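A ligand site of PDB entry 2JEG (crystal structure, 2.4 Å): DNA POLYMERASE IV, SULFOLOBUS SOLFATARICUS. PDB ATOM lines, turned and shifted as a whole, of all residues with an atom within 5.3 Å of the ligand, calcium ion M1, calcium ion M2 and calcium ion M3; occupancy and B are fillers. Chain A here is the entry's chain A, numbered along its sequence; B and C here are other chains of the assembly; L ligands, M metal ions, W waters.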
ATOM      1  N   ASP A  13     -33.534  24.423 -20.047  1.00  0.00           N
ATOM      2  CA  ASP A  13     -32.860  24.635 -18.766  1.00  0.00           C
ATOM      3  C   ASP A  13     -31.775  23.545 -18.678  1.00  0.00           C
ATOM      4  O   ASP A  13     -32.100  22.368 -18.698  1.00  0.00           O
ATOM      5  CB  ASP A  13     -33.861  24.491 -17.613  1.00  0.00           C
ATOM      6  CG  ASP A  13     -33.373  25.133 -16.339  1.00  0.00           C
ATOM      7  OD1 ASP A  13     -34.125  25.184 -15.342  1.00  0.00           O
ATOM      8  OD2 ASP A  13     -32.228  25.599 -16.336  1.00  0.00           O
ATOM      9  N   PHE A  14     -30.502  23.945 -18.591  1.00  0.00           N
ATOM     10  CA  PHE A  14     -29.396  22.967 -18.539  1.00  0.00           C
ATOM     11  C   PHE A  14     -29.335  22.184 -17.223  1.00  0.00           C
ATOM     12  O   PHE A  14     -29.295  22.778 -16.176  1.00  0.00           O
ATOM     13  CB  PHE A  14     -28.039  23.663 -18.745  1.00  0.00           C
ATOM     14  CG  PHE A  14     -28.000  24.642 -19.882  1.00  0.00           C
ATOM     15  CD1 PHE A  14     -28.899  24.560 -20.942  1.00  0.00           C
ATOM     16  CD2 PHE A  14     -27.041  25.663 -19.905  1.00  0.00           C
ATOM     17  CE1 PHE A  14     -28.854  25.475 -22.009  1.00  0.00           C
ATOM     18  CE2 PHE A  14     -27.003  26.583 -20.966  1.00  0.00           C
ATOM     19  CZ  PHE A  14     -27.914  26.486 -22.013  1.00  0.00           C
ATOM     20  N   ASP A  15     -29.278  20.863 -17.277  1.00  0.00           N
ATOM     21  CA  ASP A  15     -29.249  20.060 -16.039  1.00  0.00           C
ATOM     22  C   ASP A  15     -28.022  20.266 -15.127  1.00  0.00           C
ATOM     23  O   ASP A  15     -26.903  20.213 -15.615  1.00  0.00           O
ATOM     24  CB  ASP A  15     -29.354  18.572 -16.354  1.00  0.00           C
ATOM     25  CG  ASP A  15     -30.579  18.232 -17.153  1.00  0.00           C
ATOM     26  OD1 ASP A  15     -31.645  18.857 -16.946  1.00  0.00           O
ATOM     27  OD2 ASP A  15     -30.473  17.293 -17.968  1.00  0.00           O
ATOM     28  N   TYR A  16     -28.267  20.448 -13.819  1.00  0.00           N
ATOM     29  CA  TYR A  16     -27.214  20.681 -12.811  1.00  0.00           C
ATOM     30  C   TYR A  16     -25.961  21.279 -13.462  1.00  0.00           C
ATOM     31  O   TYR A  16     -24.822  20.852 -13.212  1.00  0.00           O
ATOM     32  CB  TYR A  16     -26.895  19.380 -12.051  1.00  0.00           C
ATOM     33  CG  TYR A  16     -26.340  18.237 -12.898  1.00  0.00           C
ATOM     34  CD1 TYR A  16     -24.971  17.937 -12.884  1.00  0.00           C
ATOM     35  CD2 TYR A  16     -27.176  17.480 -13.723  1.00  0.00           C
ATOM     36  CE1 TYR A  16     -24.445  16.902 -13.668  1.00  0.00           C
ATOM     37  CE2 TYR A  16     -26.663  16.443 -14.522  1.00  0.00           C
ATOM     38  CZ  TYR A  16     -25.286  16.163 -14.478  1.00  0.00           C
ATOM     39  OH  TYR A  16     -24.769  15.128 -15.240  1.00  0.00           O
ATOM     40  N   PHE A  17     -26.193  22.313 -14.259  1.00  0.00           N
ATOM     41  CA  PHE A  17     -25.185  22.971 -15.065  1.00  0.00           C
ATOM     42  C   PHE A  17     -23.738  23.119 -14.623  1.00  0.00           C
ATOM     43  O   PHE A  17     -22.857  22.573 -15.271  1.00  0.00           O
ATOM     44  CB  PHE A  17     -25.692  24.341 -15.534  1.00  0.00           C
ATOM     45  CG  PHE A  17     -24.896  24.910 -16.663  1.00  0.00           C
ATOM     46  CD1 PHE A  17     -24.642  24.137 -17.810  1.00  0.00           C
ATOM     47  CD2 PHE A  17     -24.380  26.196 -16.602  1.00  0.00           C
ATOM     48  CE1 PHE A  17     -23.887  24.655 -18.868  1.00  0.00           C
ATOM     49  CE2 PHE A  17     -23.629  26.722 -17.671  1.00  0.00           C
ATOM     50  CZ  PHE A  17     -23.385  25.949 -18.796  1.00  0.00           C
ATOM     51  N   TYR A  18     -23.464  23.866 -13.566  1.00  0.00           N
ATOM     52  CA  TYR A  18     -22.083  24.038 -13.136  1.00  0.00           C
ATOM     53  C   TYR A  18     -21.379  22.700 -12.914  1.00  0.00           C
ATOM     54  O   TYR A  18     -20.259  22.481 -13.406  1.00  0.00           O
ATOM     55  CB  TYR A  18     -22.023  24.840 -11.843  1.00  0.00           C
ATOM     56  CG  TYR A  18     -22.263  26.325 -11.973  1.00  0.00           C
ATOM     57  CD1 TYR A  18     -22.781  26.878 -13.158  1.00  0.00           C
ATOM     58  CD2 TYR A  18     -22.044  27.175 -10.882  1.00  0.00           C
ATOM     59  CE1 TYR A  18     -23.070  28.230 -13.238  1.00  0.00           C
ATOM     60  CE2 TYR A  18     -22.333  28.526 -10.963  1.00  0.00           C
ATOM     61  CZ  TYR A  18     -22.850  29.049 -12.143  1.00  0.00           C
ATOM     62  OH  TYR A  18     -23.171  30.381 -12.179  1.00  0.00           O
ATOM     63  N   ALA A  19     -22.020  21.814 -12.172  1.00  0.00           N
ATOM     64  CA  ALA A  19     -21.417  20.517 -11.880  1.00  0.00           C
ATOM     65  C   ALA A  19     -21.311  19.690 -13.156  1.00  0.00           C
ATOM     66  O   ALA A  19     -20.334  18.961 -13.349  1.00  0.00           O
ATOM     67  CB  ALA A  19     -22.257  19.774 -10.806  1.00  0.00           C
ATOM     68  N   VAL A  38     -18.364  27.544  -3.277  1.00  0.00           N
ATOM     69  CA  VAL A  38     -17.977  28.944  -3.265  1.00  0.00           C
ATOM     70  C   VAL A  38     -17.299  29.115  -1.915  1.00  0.00           C
ATOM     71  O   VAL A  38     -17.965  29.277  -0.889  1.00  0.00           O
ATOM     72  CB  VAL A  38     -19.218  29.870  -3.311  1.00  0.00           C
ATOM     73  CG1 VAL A  38     -18.748  31.325  -3.476  1.00  0.00           C
ATOM     74  CG2 VAL A  38     -20.137  29.480  -4.442  1.00  0.00           C
ATOM     75  N   VAL A  49     -22.617  25.946  -1.101  1.00  0.00           N
ATOM     76  CA  VAL A  49     -22.676  25.162  -2.317  1.00  0.00           C
ATOM     77  C   VAL A  49     -23.409  25.926  -3.410  1.00  0.00           C
ATOM     78  O   VAL A  49     -24.486  26.448  -3.164  1.00  0.00           O
ATOM     79  CB  VAL A  49     -23.400  23.810  -2.050  1.00  0.00           C
ATOM     80  CG1 VAL A  49     -23.637  23.059  -3.355  1.00  0.00           C
ATOM     81  CG2 VAL A  49     -22.571  22.958  -1.125  1.00  0.00           C
ATOM     82  N   ALA A  50     -22.815  26.018  -4.598  1.00  0.00           N
ATOM     83  CA  ALA A  50     -23.481  26.697  -5.724  1.00  0.00           C
ATOM     84  C   ALA A  50     -24.463  25.697  -6.302  1.00  0.00           C
ATOM     85  O   ALA A  50     -25.613  26.039  -6.611  1.00  0.00           O
ATOM     86  CB  ALA A  50     -22.446  27.115  -6.800  1.00  0.00           C
ATOM     87  N   THR A  51     -23.997  24.462  -6.464  1.00  0.00           N
ATOM     88  CA  THR A  51     -24.818  23.371  -6.971  1.00  0.00           C
ATOM     89  C   THR A  51     -24.087  22.030  -6.853  1.00  0.00           C
ATOM     90  O   THR A  51     -22.873  21.974  -6.645  1.00  0.00           O
ATOM     91  CB  THR A  51     -25.223  23.598  -8.449  1.00  0.00           C
ATOM     92  OG1 THR A  51     -26.284  22.704  -8.799  1.00  0.00           O
ATOM     93  CG2 THR A  51     -24.040  23.350  -9.382  1.00  0.00           C
ATOM     94  N   ALA A  52     -24.835  20.948  -6.995  1.00  0.00           N
ATOM     95  CA  ALA A  52     -24.243  19.617  -6.918  1.00  0.00           C
ATOM     96  C   ALA A  52     -24.920  18.785  -7.981  1.00  0.00           C
ATOM     97  O   ALA A  52     -26.003  19.154  -8.435  1.00  0.00           O
ATOM     98  CB  ALA A  52     -24.515  19.021  -5.537  1.00  0.00           C
ATOM     99  N   TYR A  54     -26.881  15.270  -9.333  1.00  0.00           N
ATOM    100  CA  TYR A  54     -27.916  14.463  -8.736  1.00  0.00           C
ATOM    101  C   TYR A  54     -27.426  13.338  -7.831  1.00  0.00           C
ATOM    102  O   TYR A  54     -28.143  12.902  -6.940  1.00  0.00           O
ATOM    103  CB  TYR A  54     -28.848  13.925  -9.833  1.00  0.00           C
ATOM    104  CG  TYR A  54     -29.729  15.009 -10.411  1.00  0.00           C
ATOM    105  CD1 TYR A  54     -29.187  15.996 -11.242  1.00  0.00           C
ATOM    106  CD2 TYR A  54     -31.074  15.110 -10.065  1.00  0.00           C
ATOM    107  CE1 TYR A  54     -29.969  17.061 -11.717  1.00  0.00           C
ATOM    108  CE2 TYR A  54     -31.867  16.160 -10.527  1.00  0.00           C
ATOM    109  CZ  TYR A  54     -31.308  17.137 -11.346  1.00  0.00           C
ATOM    110  OH  TYR A  54     -32.081  18.185 -11.800  1.00  0.00           O
ATOM    111  N   ARG A  57     -27.262  15.330  -4.802  1.00  0.00           N
ATOM    112  CA  ARG A  57     -28.561  15.820  -4.355  1.00  0.00           C
ATOM    113  C   ARG A  57     -29.406  14.759  -3.660  1.00  0.00           C
ATOM    114  O   ARG A  57     -30.177  15.074  -2.766  1.00  0.00           O
ATOM    115  CB  ARG A  57     -29.364  16.410  -5.520  1.00  0.00           C
ATOM    116  CG  ARG A  57     -29.018  17.833  -5.853  1.00  0.00           C
ATOM    117  CD  ARG A  57     -29.778  18.331  -7.056  1.00  0.00           C
ATOM    118  NE  ARG A  57     -28.941  19.228  -7.840  1.00  0.00           N
ATOM    119  CZ  ARG A  57     -29.367  19.957  -8.877  1.00  0.00           C
ATOM    120  NH1 ARG A  57     -30.638  19.885  -9.258  1.00  0.00           N
ATOM    121  NH2 ARG A  57     -28.533  20.758  -9.510  1.00  0.00           N
ATOM    122  N   ALA A  63     -27.693  23.271  -3.619  1.00  0.00           N
ATOM    123  CA  ALA A  63     -27.301  24.680  -3.641  1.00  0.00           C
ATOM    124  C   ALA A  63     -27.759  25.381  -2.384  1.00  0.00           C
ATOM    125  O   ALA A  63     -28.861  25.134  -1.893  1.00  0.00           O
ATOM    126  CB  ALA A  63     -27.900  25.353  -4.853  1.00  0.00           C
ATOM    127  N   GLY A  64     -26.900  26.252  -1.851  1.00  0.00           N
ATOM    128  CA  GLY A  64     -27.257  27.011  -0.665  1.00  0.00           C
ATOM    129  C   GLY A  64     -26.826  26.493   0.700  1.00  0.00           C
ATOM    130  O   GLY A  64     -26.755  27.278   1.635  1.00  0.00           O
ATOM    131  N   MET A  82     -15.940  26.929  -7.546  1.00  0.00           N
ATOM    132  CA  MET A  82     -16.715  27.438  -8.671  1.00  0.00           C
ATOM    133  C   MET A  82     -15.846  28.164  -9.713  1.00  0.00           C
ATOM    134  O   MET A  82     -15.039  29.024  -9.361  1.00  0.00           O
ATOM    135  CB  MET A  82     -17.813  28.364  -8.157  1.00  0.00           C
ATOM    136  CG  MET A  82     -18.489  29.162  -9.238  1.00  0.00           C
ATOM    137  SD  MET A  82     -19.918  29.987  -8.630  1.00  0.00           S
ATOM    138  CE  MET A  82     -19.209  31.544  -8.013  1.00  0.00           C
ATOM    139  N   SER A 109     -30.934  33.467 -18.317  1.00  0.00           N
ATOM    140  CA  SER A 109     -29.836  33.354 -17.378  1.00  0.00           C
ATOM    141  C   SER A 109     -28.686  32.534 -17.954  1.00  0.00           C
ATOM    142  O   SER A 109     -28.722  32.112 -19.098  1.00  0.00           O
ATOM    143  CB  SER A 109     -30.324  32.679 -16.089  1.00  0.00           C
ATOM    144  OG  SER A 109     -30.402  31.274 -16.253  1.00  0.00           O
ATOM    145  N   ILE A 110     -27.678  32.301 -17.132  1.00  0.00           N
ATOM    146  CA  ILE A 110     -26.529  31.525 -17.566  1.00  0.00           C
ATOM    147  C   ILE A 110     -26.908  30.113 -18.012  1.00  0.00           C
ATOM    148  O   ILE A 110     -26.145  29.477 -18.744  1.00  0.00           O
ATOM    149  CB  ILE A 110     -25.481  31.389 -16.430  1.00  0.00           C
ATOM    150  CG1 ILE A 110     -24.150  30.900 -17.028  1.00  0.00           C
ATOM    151  CG2 ILE A 110     -25.993  30.382 -15.339  1.00  0.00           C
ATOM    152  CD1 ILE A 110     -22.978  31.092 -16.106  1.00  0.00           C
ATOM    153  N   ASP A 111     -28.058  29.605 -17.574  1.00  0.00           N
ATOM    154  CA  ASP A 111     -28.398  28.257 -17.999  1.00  0.00           C
ATOM    155  C   ASP A 111     -29.819  28.001 -18.474  1.00  0.00           C
ATOM    156  O   ASP A 111     -30.284  26.854 -18.481  1.00  0.00           O
ATOM    157  CB  ASP A 111     -28.026  27.273 -16.889  1.00  0.00           C
ATOM    158  CG  ASP A 111     -29.156  27.018 -15.941  1.00  0.00           C
ATOM    159  OD1 ASP A 111     -29.885  27.960 -15.569  1.00  0.00           O
ATOM    160  OD2 ASP A 111     -29.287  25.856 -15.556  1.00  0.00           O
ATOM    161  N   GLU A 112     -30.518  29.052 -18.872  1.00  0.00           N
ATOM    162  CA  GLU A 112     -31.861  28.871 -19.388  1.00  0.00           C
ATOM    163  C   GLU A 112     -32.234  29.930 -20.414  1.00  0.00           C
ATOM    164  O   GLU A 112     -31.747  31.064 -20.371  1.00  0.00           O
ATOM    165  CB  GLU A 112     -32.887  28.804 -18.251  1.00  0.00           C
ATOM    166  CG  GLU A 112     -33.020  30.036 -17.376  1.00  0.00           C
ATOM    167  CD  GLU A 112     -33.963  29.801 -16.192  1.00  0.00           C
ATOM    168  OE1 GLU A 112     -34.668  30.738 -15.788  1.00  0.00           O
ATOM    169  OE2 GLU A 112     -34.014  28.681 -15.669  1.00  0.00           O
ATOM    170  N   LYS A 158     -41.699  27.041 -18.407  1.00  0.00           N
ATOM    171  CA  LYS A 158     -40.734  26.862 -17.327  1.00  0.00           C
ATOM    172  C   LYS A 158     -41.208  25.784 -16.367  1.00  0.00           C
ATOM    173  O   LYS A 158     -40.435  24.884 -16.016  1.00  0.00           O
ATOM    174  CB  LYS A 158     -40.526  28.168 -16.550  1.00  0.00           C
ATOM    175  CG  LYS A 158     -39.642  27.964 -15.326  1.00  0.00           C
ATOM    176  CD  LYS A 158     -38.934  29.232 -14.893  1.00  0.00           C
ATOM    177  CE  LYS A 158     -37.929  28.936 -13.804  1.00  0.00           C
ATOM    178  NZ  LYS A 158     -36.953  27.876 -14.203  1.00  0.00           N
ATOM    179  N   LYS A 165     -37.498  17.586 -14.932  1.00  0.00           N
ATOM    180  CA  LYS A 165     -36.094  17.485 -14.509  1.00  0.00           C
ATOM    181  C   LYS A 165     -35.754  16.140 -13.882  1.00  0.00           C
ATOM    182  O   LYS A 165     -36.524  15.603 -13.091  1.00  0.00           O
ATOM    183  CB  LYS A 165     -35.776  18.591 -13.490  1.00  0.00           C
ATOM    184  CG  LYS A 165     -35.454  19.958 -14.076  1.00  0.00           C
ATOM    185  CD  LYS A 165     -34.076  19.976 -14.724  1.00  0.00           C
ATOM    186  CE  LYS A 165     -33.683  21.401 -15.139  1.00  0.00           C
ATOM    187  NZ  LYS A 165     -32.319  21.483 -15.745  1.00  0.00           N
ATOM    188  N   PRO A 166     -34.593  15.563 -14.248  1.00  0.00           N
ATOM    189  CA  PRO A 166     -33.595  16.059 -15.197  1.00  0.00           C
ATOM    190  C   PRO A 166     -33.645  15.341 -16.552  1.00  0.00           C
ATOM    191  O   PRO A 166     -34.379  14.376 -16.724  1.00  0.00           O
ATOM    192  CB  PRO A 166     -32.296  15.805 -14.468  1.00  0.00           C
ATOM    193  CG  PRO A 166     -32.557  14.488 -13.824  1.00  0.00           C
ATOM    194  CD  PRO A 166     -33.965  14.646 -13.282  1.00  0.00           C
ATOM    195  P    DC B   4     -20.690  32.857   3.781  1.00  0.00           P
ATOM    196  OP1  DC B   4     -19.676  33.383   4.727  1.00  0.00           O
ATOM    197  OP2  DC B   4     -21.879  33.738   3.709  1.00  0.00           O
ATOM    198  O5'  DC B   4     -20.055  32.701   2.312  1.00  0.00           O
ATOM    199  C5'  DC B   4     -20.778  32.001   1.309  1.00  0.00           C
ATOM    200  C4'  DC B   4     -20.196  32.262  -0.082  1.00  0.00           C
ATOM    201  O4'  DC B   4     -21.083  31.620  -1.015  1.00  0.00           O
ATOM    202  C3'  DC B   4     -20.192  33.737  -0.509  1.00  0.00           C
ATOM    203  O3'  DC B   4     -19.285  33.888  -1.593  1.00  0.00           O
ATOM    204  C2'  DC B   4     -21.615  33.913  -1.008  1.00  0.00           C
ATOM    205  C1'  DC B   4     -21.834  32.590  -1.718  1.00  0.00           C
ATOM    206  N1   DC B   4     -23.214  32.127  -1.755  1.00  0.00           N
ATOM    207  C2   DC B   4     -23.709  31.637  -2.951  1.00  0.00           C
ATOM    208  O2   DC B   4     -22.975  31.679  -3.946  1.00  0.00           O
ATOM    209  N3   DC B   4     -24.964  31.138  -2.999  1.00  0.00           N
ATOM    210  C4   DC B   4     -25.728  31.153  -1.905  1.00  0.00           C
ATOM    211  N4   DC B   4     -26.964  30.654  -1.997  1.00  0.00           N
ATOM    212  C5   DC B   4     -25.259  31.687  -0.666  1.00  0.00           C
ATOM    213  C6   DC B   4     -24.006  32.158  -0.638  1.00  0.00           C
ATOM    214  P   BZG B   5     -18.381  35.218  -1.708  1.00  0.00           P
ATOM    215  O1P BZG B   5     -16.956  34.893  -1.485  1.00  0.00           O
ATOM    216  O2P BZG B   5     -18.862  36.231  -0.746  1.00  0.00           O
ATOM    217  O5' BZG B   5     -18.559  35.753  -3.205  1.00  0.00           O
ATOM    218  CZ1 BZG B   5     -28.345  34.091  -0.465  1.00  0.00           C
ATOM    219  CT1 BZG B   5     -29.173  33.658   0.565  1.00  0.00           C
ATOM    220  CI  BZG B   5     -30.279  32.871   0.293  1.00  0.00           C
ATOM    221  CT2 BZG B   5     -30.566  32.502  -1.025  1.00  0.00           C
ATOM    222  CZ2 BZG B   5     -29.734  32.922  -2.057  1.00  0.00           C
ATOM    223  CE  BZG B   5     -28.628  33.713  -1.772  1.00  0.00           C
ATOM    224  CW  BZG B   5     -27.776  34.081  -2.814  1.00  0.00           C
ATOM    225  OL  BZG B   5     -27.677  33.202  -3.941  1.00  0.00           O
ATOM    226  CK  BZG B   5     -26.670  33.541  -4.805  1.00  0.00           C
ATOM    227  NJ  BZG B   5     -26.787  33.175  -6.087  1.00  0.00           N
ATOM    228  CH  BZG B   5     -25.797  33.395  -6.960  1.00  0.00           C
ATOM    229  NI  BZG B   5     -25.939  33.018  -8.231  1.00  0.00           N
ATOM    230  NG  BZG B   5     -24.656  33.998  -6.570  1.00  0.00           N
ATOM    231  CF  BZG B   5     -24.498  34.382  -5.300  1.00  0.00           C
ATOM    232  CM  BZG B   5     -25.501  34.163  -4.376  1.00  0.00           C
ATOM    233  NN  BZG B   5     -25.074  34.625  -3.210  1.00  0.00           N
ATOM    234  CO  BZG B   5     -23.840  35.102  -3.382  1.00  0.00           C
ATOM    235  NE  BZG B   5     -23.479  34.939  -4.647  1.00  0.00           N
ATOM    236  CT' BZG B   5     -22.124  35.139  -5.208  1.00  0.00           C
ATOM    237  OS' BZG B   5     -21.088  34.798  -4.274  1.00  0.00           O
ATOM    238  CP' BZG B   5     -21.752  36.571  -5.619  1.00  0.00           C
ATOM    239  C5' BZG B   5     -18.621  34.879  -4.311  1.00  0.00           C
ATOM    240  C4' BZG B   5     -19.935  35.117  -5.064  1.00  0.00           C
ATOM    241  C3' BZG B   5     -20.227  36.549  -5.518  1.00  0.00           C
ATOM    242  O3' BZG B   5     -19.635  36.749  -6.800  1.00  0.00           O
ATOM    243  P    DC C  13     -38.779  32.538  -7.046  1.00  0.00           P
ATOM    244  OP1  DC C  13     -39.716  31.868  -7.971  1.00  0.00           O
ATOM    245  OP2  DC C  13     -38.928  32.041  -5.668  1.00  0.00           O
ATOM    246  O5'  DC C  13     -37.247  32.295  -7.496  1.00  0.00           O
ATOM    247  C5'  DC C  13     -36.785  32.633  -8.792  1.00  0.00           C
ATOM    248  C4'  DC C  13     -35.324  32.195  -8.934  1.00  0.00           C
ATOM    249  O4'  DC C  13     -34.472  33.225  -8.365  1.00  0.00           O
ATOM    250  C3'  DC C  13     -35.038  30.883  -8.171  1.00  0.00           C
ATOM    251  O3'  DC C  13     -34.307  29.942  -8.975  1.00  0.00           O
ATOM    252  C2'  DC C  13     -34.205  31.347  -6.988  1.00  0.00           C
ATOM    253  C1'  DC C  13     -33.515  32.576  -7.543  1.00  0.00           C
ATOM    254  N1   DC C  13     -33.042  33.519  -6.531  1.00  0.00           N
ATOM    255  C2   DC C  13     -32.031  34.426  -6.879  1.00  0.00           C
ATOM    256  O2   DC C  13     -31.703  34.533  -8.061  1.00  0.00           O
ATOM    257  N3   DC C  13     -31.454  35.170  -5.914  1.00  0.00           N
ATOM    258  C4   DC C  13     -31.872  35.061  -4.652  1.00  0.00           C
ATOM    259  N4   DC C  13     -31.220  35.762  -3.721  1.00  0.00           N
ATOM    260  C5   DC C  13     -32.967  34.218  -4.279  1.00  0.00           C
ATOM    261  C6   DC C  13     -33.514  33.477  -5.243  1.00  0.00           C
ATOM    262  N1  DOC C  14     -34.799  34.397 -12.909  1.00  0.00           N
ATOM    263  C2  DOC C  14     -35.361  35.542 -13.429  1.00  0.00           C
ATOM    264  N3  DOC C  14     -35.751  36.553 -12.616  1.00  0.00           N
ATOM    265  C4  DOC C  14     -35.604  36.470 -11.279  1.00  0.00           C
ATOM    266  C5  DOC C  14     -35.037  35.310 -10.708  1.00  0.00           C
ATOM    267  C6  DOC C  14     -34.640  34.295 -11.527  1.00  0.00           C
ATOM    268  O2  DOC C  14     -35.515  35.662 -14.643  1.00  0.00           O
ATOM    269  N4  DOC C  14     -36.008  37.515 -10.472  1.00  0.00           N
ATOM    270  C1' DOC C  14     -34.326  33.273 -13.820  1.00  0.00           C
ATOM    271  C2' DOC C  14     -32.817  33.427 -13.757  1.00  0.00           C
ATOM    272  C3' DOC C  14     -32.301  32.159 -13.069  1.00  0.00           C
ATOM    273  C4' DOC C  14     -33.463  31.121 -13.026  1.00  0.00           C
ATOM    274  O4' DOC C  14     -34.665  31.963 -13.296  1.00  0.00           O
ATOM    275  C5' DOC C  14     -33.747  30.635 -11.650  1.00  0.00           C
ATOM    276  O5' DOC C  14     -34.662  29.551 -11.737  1.00  0.00           O
ATOM    277  P   DOC C  14     -35.050  29.272 -10.233  1.00  0.00           P
ATOM    278  OP1 DOC C  14     -36.162  30.245 -10.186  1.00  0.00           O
ATOM    279  OP2 DOC C  14     -35.837  28.042 -10.009  1.00  0.00           O
HETATM  280  P1  LIG L   1     -31.148  21.678 -12.076  1.00  0.00           P
HETATM  281  O1  LIG L   1     -32.266  21.447 -10.940  1.00  0.00           O
HETATM  282  O2  LIG L   1     -31.722  22.893 -12.973  1.00  0.00           O
HETATM  283  O3  LIG L   1     -30.919  20.460 -12.877  1.00  0.00           O
HETATM  284  O4  LIG L   1     -29.837  22.180 -11.284  1.00  0.00           O
HETATM  285  P2  LIG L   1     -28.862  23.375 -11.738  1.00  0.00           P
HETATM  286  O5  LIG L   1     -28.975  23.906 -13.117  1.00  0.00           O
HETATM  287  O6  LIG L   1     -27.630  23.446 -10.918  1.00  0.00           O
HETATM  288  O7  LIG L   1     -29.714  24.474 -10.916  1.00  0.00           O
HETATM  289  P3  LIG L   1     -30.376  25.815 -11.539  1.00  0.00           P
HETATM  290  O8  LIG L   1     -31.470  26.261 -10.459  1.00  0.00           O
HETATM  291  O9  LIG L   1     -31.007  25.610 -12.859  1.00  0.00           O
HETATM  292  O10 LIG L   1     -29.232  26.951 -11.569  1.00  0.00           O
HETATM  293  C1  LIG L   1     -28.270  26.965 -12.628  1.00  0.00           C
HETATM  294  C2  LIG L   1     -26.876  27.319 -12.115  1.00  0.00           C
HETATM  295  O11 LIG L   1     -26.833  28.621 -11.488  1.00  0.00           O
HETATM  296  C3  LIG L   1     -26.373  26.352 -11.044  1.00  0.00           C
HETATM  297  O12 LIG L   1     -25.845  25.194 -11.689  1.00  0.00           O
HETATM  298  C4  LIG L   1     -25.198  27.190 -10.532  1.00  0.00           C
HETATM  299  C5  LIG L   1     -25.859  28.572 -10.435  1.00  0.00           C
HETATM  300  N1  LIG L   1     -26.578  28.705  -9.142  1.00  0.00           N
HETATM  301  C6  LIG L   1     -27.832  28.315  -8.898  1.00  0.00           C
HETATM  302  N2  LIG L   1     -28.123  28.572  -7.628  1.00  0.00           N
HETATM  303  C7  LIG L   1     -27.050  29.127  -7.063  1.00  0.00           C
HETATM  304  C8  LIG L   1     -26.792  29.581  -5.772  1.00  0.00           C
HETATM  305  O13 LIG L   1     -27.628  29.483  -4.880  1.00  0.00           O
HETATM  306  N3  LIG L   1     -25.532  30.133  -5.494  1.00  0.00           N
HETATM  307  C9  LIG L   1     -24.567  30.212  -6.524  1.00  0.00           C
HETATM  308  N4  LIG L   1     -23.388  30.771  -6.283  1.00  0.00           N
HETATM  309  N5  LIG L   1     -24.871  29.751  -7.747  1.00  0.00           N
HETATM  310  C10 LIG L   1     -26.069  29.215  -8.029  1.00  0.00           C
HETATM  311 CA    CA M   1     -32.285  27.494 -14.295  1.00  0.00          CA
HETATM  312 CA    CA M   2     -30.693  24.182 -14.714  1.00  0.00          CA
HETATM  313 CA    CA M   3     -32.295  27.596  -8.499  1.00  0.00          CA
HETATM  314  O   HOH W   1     -30.754  29.538 -13.257  1.00  0.00           O
HETATM  315  O   HOH W   2     -23.581  31.244  -9.791  1.00  0.00           O
HETATM  316  O   HOH W   3     -30.135  28.537  -3.667  1.00  0.00           O
HETATM  317  O   HOH W   4     -34.075  25.237  -9.053  1.00  0.00           O
HETATM  318  O   HOH W   5     -34.536  27.151 -13.845  1.00  0.00           O
HETATM  319  O   HOH W   6     -30.828  24.606  -7.886  1.00  0.00           O
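O2 of DC 4 of chain B lies within hydrogen-bond range of N4 of the ligand (2.5 Å). OG1 of Thr 51 lies within hydrogen-bond range of O6 of the ligand (2.6 Å). The guanidinium group of Arg 57 is in salt-bridge range of an oxygen (O1) of the ligand (2.8 Å). OH of Tyr 54 lies within hydrogen-bond range of O3 of the ligand, 2.8 Å away. The backbone NH of Tyr 16 sits at hydrogen-bond distance from an oxygen (O3) of the ligand (2.8 Å). An oxygen (O3) of the ligand is in salt-bridge range of the side-chain amino group (NZ) of Lys 165, at 3.4 Å. The backbone NH (N) of Tyr 18 sits at hydrogen-bond distance from an oxygen (O12) of the ligand (3.3 Å). NJ of BZG 5 of chain B sits at hydrogen-bond distance from N3 of the ligand, at 3.3 Å. An oxygen (O5) of the ligand sits close to the backbone NH (N) of Phe 17 (3.4 Å).
N of Asp 111 lies close to OG of Ser 109, at 3.2 Å. The backbone carbonyl oxygen (O) of Phe 14 of chain A lies close to the side-chain amino group (NZ) of Lys 165, at 3.3 Å. OG of Ser 109 lies close to N of Glu 112 (3.4 Å). OE1 of Glu 112 is in salt-bridge range of NZ of Lys 158, 3.99 Å away. The guanidinium group of Arg 57 lies within hydrogen-bond range of the side-chain hydroxyl of Thr 51, at 3.1 Å. The guanidinium group of Arg 57 lies within hydrogen-bond range of the side-chain hydroxyl of Tyr 54 (3.4 Å). The backbone carbonyl oxygen of Ala 52 lies within hydrogen-bond range of the guanidinium group of Arg 57 (3.0 Å). NZ of Lys 165 is in hydrogen-bond range of O of Asp 13 of chain A (3.1 Å).
CA of Asp 15 touches O3 of the ligand, at 3.6 Å. Val 38 touches the ligand. Ala 50 touches the ligand. Hydrophobic or aromatic side chains within 4 Å of the ligand: Phe 17, Tyr 18, Val 38, Ala 50 and Tyr 54. Of the 28 residues printed, 15 come within 4 Å of the ligand.
Of the 28 residues printed, 3 come within 4 Å of calcium ion M1.
NZ of Lys 165 touches calcium ion M2, at 3.3 Å. Of the 28 residues printed, 4 come within 4 Å of calcium ion M2.
Residues that only touch calcium ion M3: DOC 14 of chain C (3.7 Å).
Calcium ion M1 is bound by water W5, the side-chain carboxylate (OE2) of Glu 112, an oxygen (O9) of the ligand, the side-chain carboxylate (OD1) of Asp 111, water W1 and the side-chain carboxylate (OD2) of Asp 13 of chain A. Slightly farther from calcium ion M1 lies the side-chain carboxylate (OD1) of Asp 13 of chain A (3.1 Å).
Calcium ion M2 is bound by OD2 of Asp 111 (2.3 Å), O9 of the ligand (2.4 Å), O5 of the ligand (2.4 Å), O2 of the ligand (2.4 Å), O of Phe 14 of chain A (2.5 Å) and OD2 of Asp 13 of chain A (2.6 Å).
Calcium ion M3 is bound by an oxygen (O8) of the ligand, at 2.5 Å. Slightly farther from calcium ion M3 lies water W4 (3.0 Å). Slightly farther from calcium ion M3 lies O3' of DC 13 of chain C (3.1 Å).
Water W5 lies within hydrogen-bond range of OD1 of Asp 13 of chain A (2.5 Å), NZ of Lys 158 (2.5 Å) and O5' of DOC 14 of chain C (3.2 Å). Water W1 lies within hydrogen-bond range of an oxygen (O10) of the ligand (3.4 Å) and the side-chain hydroxyl of Ser 109 (3.5 Å). Water W2 lies within hydrogen-bond range of the side-chain hydroxyl of Tyr 18 (2.6 Å), a nitrogen (N5) of the ligand (2.8 Å) and NI of BZG 5 of chain B (3.3 Å).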
